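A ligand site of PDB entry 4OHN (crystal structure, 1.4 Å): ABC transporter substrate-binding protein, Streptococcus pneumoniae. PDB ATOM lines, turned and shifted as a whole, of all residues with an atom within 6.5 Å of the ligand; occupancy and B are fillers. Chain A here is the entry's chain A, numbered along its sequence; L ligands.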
ATOM      1  N   PHE A  24     -15.681  27.419 -11.778  1.00  0.00           N
ATOM      2  CA  PHE A  24     -15.647  26.299 -10.839  1.00  0.00           C
ATOM      3  C   PHE A  24     -15.555  26.781  -9.414  1.00  0.00           C
ATOM      4  O   PHE A  24     -14.997  27.829  -9.140  1.00  0.00           O
ATOM      5  CB  PHE A  24     -14.507  25.304 -11.175  1.00  0.00           C
ATOM      6  CG  PHE A  24     -13.114  25.830 -10.905  1.00  0.00           C
ATOM      7  CD1 PHE A  24     -12.598  26.923 -11.580  1.00  0.00           C
ATOM      8  CD2 PHE A  24     -12.332  25.223  -9.943  1.00  0.00           C
ATOM      9  CE1 PHE A  24     -11.318  27.399 -11.290  1.00  0.00           C
ATOM     10  CE2 PHE A  24     -11.060  25.701  -9.659  1.00  0.00           C
ATOM     11  CZ  PHE A  24     -10.577  26.781 -10.331  1.00  0.00           C
ATOM     12  N   ASP A  25     -16.100  25.979  -8.503  1.00  0.00           N
ATOM     13  CA  ASP A  25     -15.903  26.120  -7.063  1.00  0.00           C
ATOM     14  C   ASP A  25     -14.532  25.497  -6.769  1.00  0.00           C
ATOM     15  O   ASP A  25     -14.373  24.280  -6.886  1.00  0.00           O
ATOM     16  CB  ASP A  25     -17.042  25.331  -6.367  1.00  0.00           C
ATOM     17  CG  ASP A  25     -16.876  25.128  -4.861  1.00  0.00           C
ATOM     18  OD1 ASP A  25     -15.829  25.509  -4.253  1.00  0.00           O
ATOM     19  OD2 ASP A  25     -17.818  24.521  -4.280  1.00  0.00           O
ATOM     20  N   THR A  27     -12.989  24.715  -4.234  1.00  0.00           N
ATOM     21  CA  THR A  27     -12.858  23.753  -3.146  1.00  0.00           C
ATOM     22  C   THR A  27     -13.419  22.381  -3.496  1.00  0.00           C
ATOM     23  O   THR A  27     -13.322  21.481  -2.671  1.00  0.00           O
ATOM     24  CB  THR A  27     -13.562  24.220  -1.859  1.00  0.00           C
ATOM     25  OG1 THR A  27     -14.992  24.233  -2.005  1.00  0.00           O
ATOM     26  CG2 THR A  27     -13.106  25.578  -1.417  1.00  0.00           C
ATOM     27  N   PHE A  28     -14.010  22.198  -4.675  1.00  0.00           N
ATOM     28  CA  PHE A  28     -14.792  20.982  -4.908  1.00  0.00           C
ATOM     29  C   PHE A  28     -13.925  19.797  -5.370  1.00  0.00           C
ATOM     30  O   PHE A  28     -13.813  19.486  -6.559  1.00  0.00           O
ATOM     31  CB  PHE A  28     -15.951  21.248  -5.868  1.00  0.00           C
ATOM     32  CG  PHE A  28     -16.994  20.157  -5.832  1.00  0.00           C
ATOM     33  CD1 PHE A  28     -17.888  20.066  -4.794  1.00  0.00           C
ATOM     34  CD2 PHE A  28     -17.066  19.203  -6.829  1.00  0.00           C
ATOM     35  CE1 PHE A  28     -18.829  19.062  -4.730  1.00  0.00           C
ATOM     36  CE2 PHE A  28     -18.005  18.191  -6.771  1.00  0.00           C
ATOM     37  CZ  PHE A  28     -18.890  18.118  -5.719  1.00  0.00           C
ATOM     38  N   TRP A  66     -19.944  29.700  -5.920  1.00  0.00           N
ATOM     39  CA  TRP A  66     -20.872  28.686  -6.447  1.00  0.00           C
ATOM     40  C   TRP A  66     -22.308  29.208  -6.405  1.00  0.00           C
ATOM     41  O   TRP A  66     -23.113  28.831  -7.267  1.00  0.00           O
ATOM     42  CB  TRP A  66     -20.718  27.363  -5.703  1.00  0.00           C
ATOM     43  CG  TRP A  66     -21.341  26.185  -6.372  1.00  0.00           C
ATOM     44  CD1 TRP A  66     -22.366  25.414  -5.912  1.00  0.00           C
ATOM     45  CD2 TRP A  66     -20.950  25.622  -7.641  1.00  0.00           C
ATOM     46  NE1 TRP A  66     -22.661  24.419  -6.812  1.00  0.00           N
ATOM     47  CE2 TRP A  66     -21.787  24.511  -7.875  1.00  0.00           C
ATOM     48  CE3 TRP A  66     -19.974  25.947  -8.577  1.00  0.00           C
ATOM     49  CZ2 TRP A  66     -21.683  23.740  -9.011  1.00  0.00           C
ATOM     50  CZ3 TRP A  66     -19.867  25.168  -9.719  1.00  0.00           C
ATOM     51  CH2 TRP A  66     -20.709  24.072  -9.941  1.00  0.00           C
ATOM     52  N   LYS A  69     -23.148  31.024  -9.894  1.00  0.00           N
ATOM     53  CA  LYS A  69     -22.739  30.381 -11.138  1.00  0.00           C
ATOM     54  C   LYS A  69     -23.653  30.661 -12.317  1.00  0.00           C
ATOM     55  O   LYS A  69     -23.167  30.912 -13.404  1.00  0.00           O
ATOM     56  CB  LYS A  69     -22.554  28.876 -10.934  1.00  0.00           C
ATOM     57  CG  LYS A  69     -23.791  28.148 -10.522  1.00  0.00           C
ATOM     58  CD  LYS A  69     -23.449  26.777 -10.004  1.00  0.00           C
ATOM     59  CE  LYS A  69     -24.612  26.112  -9.288  1.00  0.00           C
ATOM     60  NZ  LYS A  69     -25.003  26.870  -8.063  1.00  0.00           N
ATOM     61  N   ASN A  83     -17.408  21.440 -13.033  1.00  0.00           N
ATOM     62  CA  ASN A  83     -16.942  21.263 -11.643  1.00  0.00           C
ATOM     63  C   ASN A  83     -17.893  20.350 -10.906  1.00  0.00           C
ATOM     64  O   ASN A  83     -18.559  20.754  -9.947  1.00  0.00           O
ATOM     65  CB  ASN A  83     -16.890  22.628 -10.954  1.00  0.00           C
ATOM     66  CG  ASN A  83     -16.303  22.615  -9.557  1.00  0.00           C
ATOM     67  OD1 ASN A  83     -16.985  23.024  -8.610  1.00  0.00           O
ATOM     68  ND2 ASN A  83     -15.052  22.205  -9.433  1.00  0.00           N
ATOM     69  N   GLY A  84     -17.977  19.103 -11.316  1.00  0.00           N
ATOM     70  CA  GLY A  84     -18.978  18.224 -10.718  1.00  0.00           C
ATOM     71  C   GLY A  84     -20.359  18.840 -10.735  1.00  0.00           C
ATOM     72  O   GLY A  84     -21.075  18.803  -9.730  1.00  0.00           O
ATOM     73  N   TYR A  85     -20.730  19.397 -11.889  1.00  0.00           N
ATOM     74  CA  TYR A  85     -21.968  20.143 -12.011  1.00  0.00           C
ATOM     75  C   TYR A  85     -23.109  19.163 -12.320  1.00  0.00           C
ATOM     76  O   TYR A  85     -23.179  18.586 -13.416  1.00  0.00           O
ATOM     77  CB  TYR A  85     -21.826  21.210 -13.095  1.00  0.00           C
ATOM     78  CG  TYR A  85     -22.950  22.213 -13.245  1.00  0.00           C
ATOM     79  CD1 TYR A  85     -23.604  22.772 -12.164  1.00  0.00           C
ATOM     80  CD2 TYR A  85     -23.300  22.656 -14.511  1.00  0.00           C
ATOM     81  CE1 TYR A  85     -24.593  23.739 -12.332  1.00  0.00           C
ATOM     82  CE2 TYR A  85     -24.285  23.607 -14.692  1.00  0.00           C
ATOM     83  CZ  TYR A  85     -24.926  24.140 -13.606  1.00  0.00           C
ATOM     84  OH  TYR A  85     -25.897  25.076 -13.828  1.00  0.00           O
ATOM     85  N   SER A  86     -24.011  18.978 -11.364  1.00  0.00           N
ATOM     86  CA  SER A  86     -25.097  17.997 -11.509  1.00  0.00           C
ATOM     87  C   SER A  86     -26.144  18.469 -12.499  1.00  0.00           C
ATOM     88  O   SER A  86     -26.664  19.585 -12.390  1.00  0.00           O
ATOM     89  CB  SER A  86     -25.737  17.759 -10.155  1.00  0.00           C
ATOM     90  OG  SER A  86     -24.746  17.274  -9.249  1.00  0.00           O
ATOM     91  N   ALA A  87     -26.451  17.602 -13.460  1.00  0.00           N
ATOM     92  CA  ALA A  87     -27.409  17.907 -14.523  1.00  0.00           C
ATOM     93  C   ALA A  87     -28.801  17.568 -14.072  1.00  0.00           C
ATOM     94  O   ALA A  87     -29.244  16.419 -14.168  1.00  0.00           O
ATOM     95  CB  ALA A  87     -27.055  17.133 -15.791  1.00  0.00           C
ATOM     96  N   ARG A  91     -32.129  22.779 -13.492  1.00  0.00           N
ATOM     97  CA  ARG A  91     -31.076  23.524 -14.166  1.00  0.00           C
ATOM     98  C   ARG A  91     -31.248  23.546 -15.680  1.00  0.00           C
ATOM     99  O   ARG A  91     -30.823  24.501 -16.336  1.00  0.00           O
ATOM    100  CB  ARG A  91     -29.714  22.949 -13.788  1.00  0.00           C
ATOM    101  CG  ARG A  91     -29.353  23.287 -12.365  1.00  0.00           C
ATOM    102  CD  ARG A  91     -28.127  22.579 -11.876  1.00  0.00           C
ATOM    103  NE  ARG A  91     -27.694  23.108 -10.592  1.00  0.00           N
ATOM    104  CZ  ARG A  91     -26.739  22.573  -9.848  1.00  0.00           C
ATOM    105  NH1 ARG A  91     -26.131  21.471 -10.230  1.00  0.00           N
ATOM    106  NH2 ARG A  91     -26.400  23.173  -8.714  1.00  0.00           N
ATOM    107  N   ASN A 104     -23.163  10.340  -9.865  1.00  0.00           N
ATOM    108  CA  ASN A 104     -22.915  10.866  -8.533  1.00  0.00           C
ATOM    109  C   ASN A 104     -24.145  10.623  -7.690  1.00  0.00           C
ATOM    110  O   ASN A 104     -25.230  10.400  -8.213  1.00  0.00           O
ATOM    111  CB  ASN A 104     -22.616  12.362  -8.633  1.00  0.00           C
ATOM    112  CG  ASN A 104     -22.332  13.011  -7.289  1.00  0.00           C
ATOM    113  OD1 ASN A 104     -21.457  12.555  -6.509  1.00  0.00           O
ATOM    114  ND2 ASN A 104     -23.151  14.010  -6.972  1.00  0.00           N
ATOM    115  N   GLN A 106     -26.015  11.952  -3.818  1.00  0.00           N
ATOM    116  CA  GLN A 106     -26.024  12.764  -2.617  1.00  0.00           C
ATOM    117  C   GLN A 106     -26.058  11.846  -1.400  1.00  0.00           C
ATOM    118  O   GLN A 106     -26.841  10.876  -1.319  1.00  0.00           O
ATOM    119  CB  GLN A 106     -27.206  13.727  -2.627  1.00  0.00           C
ATOM    120  CG  GLN A 106     -27.189  14.707  -3.811  1.00  0.00           C
ATOM    121  CD  GLN A 106     -26.060  15.710  -3.727  1.00  0.00           C
ATOM    122  OE1 GLN A 106     -25.744  16.240  -2.663  1.00  0.00           O
ATOM    123  NE2 GLN A 106     -25.408  15.954  -4.859  1.00  0.00           N
ATOM    124  N   GLN A 130     -24.484  22.768   1.258  1.00  0.00           N
ATOM    125  CA  GLN A 130     -23.927  23.854   0.444  1.00  0.00           C
ATOM    126  C   GLN A 130     -25.066  24.612  -0.217  1.00  0.00           C
ATOM    127  O   GLN A 130     -25.922  24.033  -0.888  1.00  0.00           O
ATOM    128  CB  GLN A 130     -22.960  23.321  -0.620  1.00  0.00           C
ATOM    129  CG  GLN A 130     -22.418  24.452  -1.477  1.00  0.00           C
ATOM    130  CD  GLN A 130     -21.482  23.998  -2.583  1.00  0.00           C
ATOM    131  OE1 GLN A 130     -21.772  23.032  -3.324  1.00  0.00           O
ATOM    132  NE2 GLN A 130     -20.364  24.693  -2.742  1.00  0.00           N
ATOM    133  N   GLY A 132     -25.569  26.645  -2.676  1.00  0.00           N
ATOM    134  CA  GLY A 132     -25.782  26.665  -4.123  1.00  0.00           C
ATOM    135  C   GLY A 132     -25.826  25.286  -4.761  1.00  0.00           C
ATOM    136  O   GLY A 132     -25.808  25.160  -5.981  1.00  0.00           O
ATOM    137  N   SER A 133     -25.857  24.254  -3.935  1.00  0.00           N
ATOM    138  CA  SER A 133     -25.751  22.880  -4.443  1.00  0.00           C
ATOM    139  C   SER A 133     -27.057  22.265  -4.913  1.00  0.00           C
ATOM    140  O   SER A 133     -28.148  22.608  -4.467  1.00  0.00           O
ATOM    141  CB  SER A 133     -25.148  21.969  -3.391  1.00  0.00           C
ATOM    142  OG  SER A 133     -26.039  21.703  -2.319  1.00  0.00           O
ATOM    143  N   SER A 134     -26.917  21.305  -5.795  1.00  0.00           N
ATOM    144  CA  SER A 134     -28.048  20.506  -6.252  1.00  0.00           C
ATOM    145  C   SER A 134     -28.607  19.712  -5.052  1.00  0.00           C
ATOM    146  O   SER A 134     -29.795  19.452  -4.991  1.00  0.00           O
ATOM    147  CB  SER A 134     -27.608  19.586  -7.394  1.00  0.00           C
ATOM    148  OG  SER A 134     -26.503  18.833  -7.007  1.00  0.00           O
ATOM    149  N   GLY A 135     -27.751  19.323  -4.134  1.00  0.00           N
ATOM    150  CA  GLY A 135     -28.203  18.632  -2.939  1.00  0.00           C
ATOM    151  C   GLY A 135     -29.188  19.459  -2.138  1.00  0.00           C
ATOM    152  O   GLY A 135     -30.234  18.933  -1.707  1.00  0.00           O
ATOM    153  N   PHE A 161     -18.327  23.318   0.874  1.00  0.00           N
ATOM    154  CA  PHE A 161     -18.378  22.129   1.705  1.00  0.00           C
ATOM    155  C   PHE A 161     -17.258  22.089   2.749  1.00  0.00           C
ATOM    156  O   PHE A 161     -17.446  21.487   3.820  1.00  0.00           O
ATOM    157  CB  PHE A 161     -18.358  20.887   0.814  1.00  0.00           C
ATOM    158  CG  PHE A 161     -19.693  20.583   0.186  1.00  0.00           C
ATOM    159  CD1 PHE A 161     -20.803  20.339   0.976  1.00  0.00           C
ATOM    160  CD2 PHE A 161     -19.824  20.513  -1.188  1.00  0.00           C
ATOM    161  CE1 PHE A 161     -22.013  20.016   0.399  1.00  0.00           C
ATOM    162  CE2 PHE A 161     -21.038  20.206  -1.752  1.00  0.00           C
ATOM    163  CZ  PHE A 161     -22.122  19.977  -0.971  1.00  0.00           C
ATOM    164  N   ASP A 179     -22.158  15.694  -1.952  1.00  0.00           N
ATOM    165  CA  ASP A 179     -21.824  14.767  -3.012  1.00  0.00           C
ATOM    166  C   ASP A 179     -20.914  13.648  -2.529  1.00  0.00           C
ATOM    167  O   ASP A 179     -19.915  13.885  -1.876  1.00  0.00           O
ATOM    168  CB  ASP A 179     -21.127  15.517  -4.157  1.00  0.00           C
ATOM    169  CG  ASP A 179     -21.934  16.666  -4.656  1.00  0.00           C
ATOM    170  OD1 ASP A 179     -22.084  17.641  -3.908  1.00  0.00           O
ATOM    171  OD2 ASP A 179     -22.414  16.588  -5.793  1.00  0.00           O
ATOM    172  N   GLU A 206     -27.582  11.280  -9.377  1.00  0.00           N
ATOM    173  CA  GLU A 206     -27.283  12.394 -10.254  1.00  0.00           C
ATOM    174  C   GLU A 206     -26.259  11.925 -11.310  1.00  0.00           C
ATOM    175  O   GLU A 206     -25.646  10.844 -11.203  1.00  0.00           O
ATOM    176  CB  GLU A 206     -26.708  13.582  -9.453  1.00  0.00           C
ATOM    177  CG  GLU A 206     -27.698  14.333  -8.513  1.00  0.00           C
ATOM    178  CD  GLU A 206     -27.050  15.463  -7.713  1.00  0.00           C
ATOM    179  OE1 GLU A 206     -25.807  15.458  -7.628  1.00  0.00           O
ATOM    180  OE2 GLU A 206     -27.762  16.354  -7.195  1.00  0.00           O
ATOM    181  N   PHE A 208     -23.045  14.110 -13.527  1.00  0.00           N
ATOM    182  CA  PHE A 208     -22.315  15.327 -13.812  1.00  0.00           C
ATOM    183  C   PHE A 208     -22.250  15.567 -15.309  1.00  0.00           C
ATOM    184  O   PHE A 208     -22.079  14.634 -16.100  1.00  0.00           O
ATOM    185  CB  PHE A 208     -20.872  15.219 -13.307  1.00  0.00           C
ATOM    186  CG  PHE A 208     -20.699  15.140 -11.803  1.00  0.00           C
ATOM    187  CD1 PHE A 208     -21.611  15.672 -10.911  1.00  0.00           C
ATOM    188  CD2 PHE A 208     -19.539  14.573 -11.283  1.00  0.00           C
ATOM    189  CE1 PHE A 208     -21.398  15.615  -9.548  1.00  0.00           C
ATOM    190  CE2 PHE A 208     -19.326  14.516  -9.921  1.00  0.00           C
ATOM    191  CZ  PHE A 208     -20.246  15.031  -9.059  1.00  0.00           C
HETATM  192  N1  LIG L   1     -22.839  18.609  -7.537  1.00  0.00           N
HETATM  193  C1  LIG L   1     -23.314  19.780  -6.772  1.00  0.00           C
HETATM  194  C2  LIG L   1     -23.840  20.849  -7.698  1.00  0.00           C
HETATM  195  O1  LIG L   1     -23.771  20.673  -8.937  1.00  0.00           O
HETATM  196  C3  LIG L   1     -22.249  20.306  -5.770  1.00  0.00           C
HETATM  197  C4  LIG L   1     -21.125  21.126  -6.349  1.00  0.00           C
HETATM  198  N2  LIG L   1     -20.594  22.195  -5.646  1.00  0.00           N
HETATM  199  C5  LIG L   1     -20.370  20.998  -7.462  1.00  0.00           C
HETATM  200  C6  LIG L   1     -19.578  22.699  -6.317  1.00  0.00           C
HETATM  201  N3  LIG L   1     -19.417  21.990  -7.428  1.00  0.00           N
HETATM  202  O2  LIG L   1     -24.330  21.875  -7.166  1.00  0.00           O
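Residues that only touch the ligand: Ser 133 (3.2 Å), Asp 25 (3.3 Å), Phe 28 (3.4 Å), Tyr 85 (3.6 Å), Gly 132 (3.8 Å) and Phe 208 (3.9 Å).
Hydrophobic or aromatic side chains within 4 Å of the ligand: Phe 28, Trp 66, Tyr 85 and Phe 208.
Within 4 Å of the ligand: Asp 25, Phe 28, Trp 66, Asn 83, Gly 84, Tyr 85, Ser 86, Arg 91, Gln 130, Gly 132, Ser 133, Ser 134, Asp 179 and Phe 208.
The nearest printed residue that does not touch the ligand is Phe 161 (4.2 Å).
The backbone NH of Ser 86 lies within hydrogen-bond range of an oxygen (O1) of the ligand (3.0 Å).
NH1 of Arg 91 lies within salt-bridge range of O1 of the ligand (2.8 Å).
The side-chain carboxylate (OD2) of Asp 179 is in salt-bridge range of a nitrogen (N1) of the ligand (2.7 Å).
An oxygen (O2) of the ligand lies within hydrogen-bond range of the indole nitrogen of Trp 66 (3.1 Å).
The backbone carbonyl oxygen (O) of Asn 83 lies within hydrogen-bond range of a nitrogen (N3) of the ligand (2.9 Å).
OD1 of Asn 83 is in hydrogen-bond range of N3 of the ligand.
A nitrogen (N1) of the ligand is in hydrogen-bond range of the backbone carbonyl oxygen of Gly 84, 2.8 Å away.
An oxygen (O2) of the ligand is in hydrogen-bond range of the backbone NH of Ser 134 (3.0 Å).
OG of Ser 86 lies within hydrogen-bond range of N1 of the ligand (2.9 Å).
OE1 of Gln 130 lies close to N2 of the ligand.
OD1 of Asn 83 lies within hydrogen-bond range of N of Asp 25, 3.1 Å away.
The backbone carbonyl oxygen of Gly 132 lies within hydrogen-bond range of the side-chain amino group of Lys 69.
The backbone carbonyl oxygen (O) of Gln 130 is in hydrogen-bond range of the side-chain hydroxyl (OG) of Ser 133 (2.7 Å).
The backbone NH (N) of Gly 135 sits close to the side-chain hydroxyl (OG) of Ser 133.
The side-chain hydroxyl (OG) of Ser 134 sits at hydrogen-bond distance from the side-chain hydroxyl (OG) of Ser 86.
The backbone carbonyl oxygen (O) of Gly 132 sits at hydrogen-bond distance from the guanidinium group (NH2) of Arg 91 (3.4 Å).
The indole nitrogen (NE1) of Trp 66 sits at hydrogen-bond distance from the backbone carbonyl oxygen (O) of Gly 132 (3.3 Å).
NE2 of Gln 130 lies within hydrogen-bond range of OD2 of Asp 25, at 3.0 Å.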
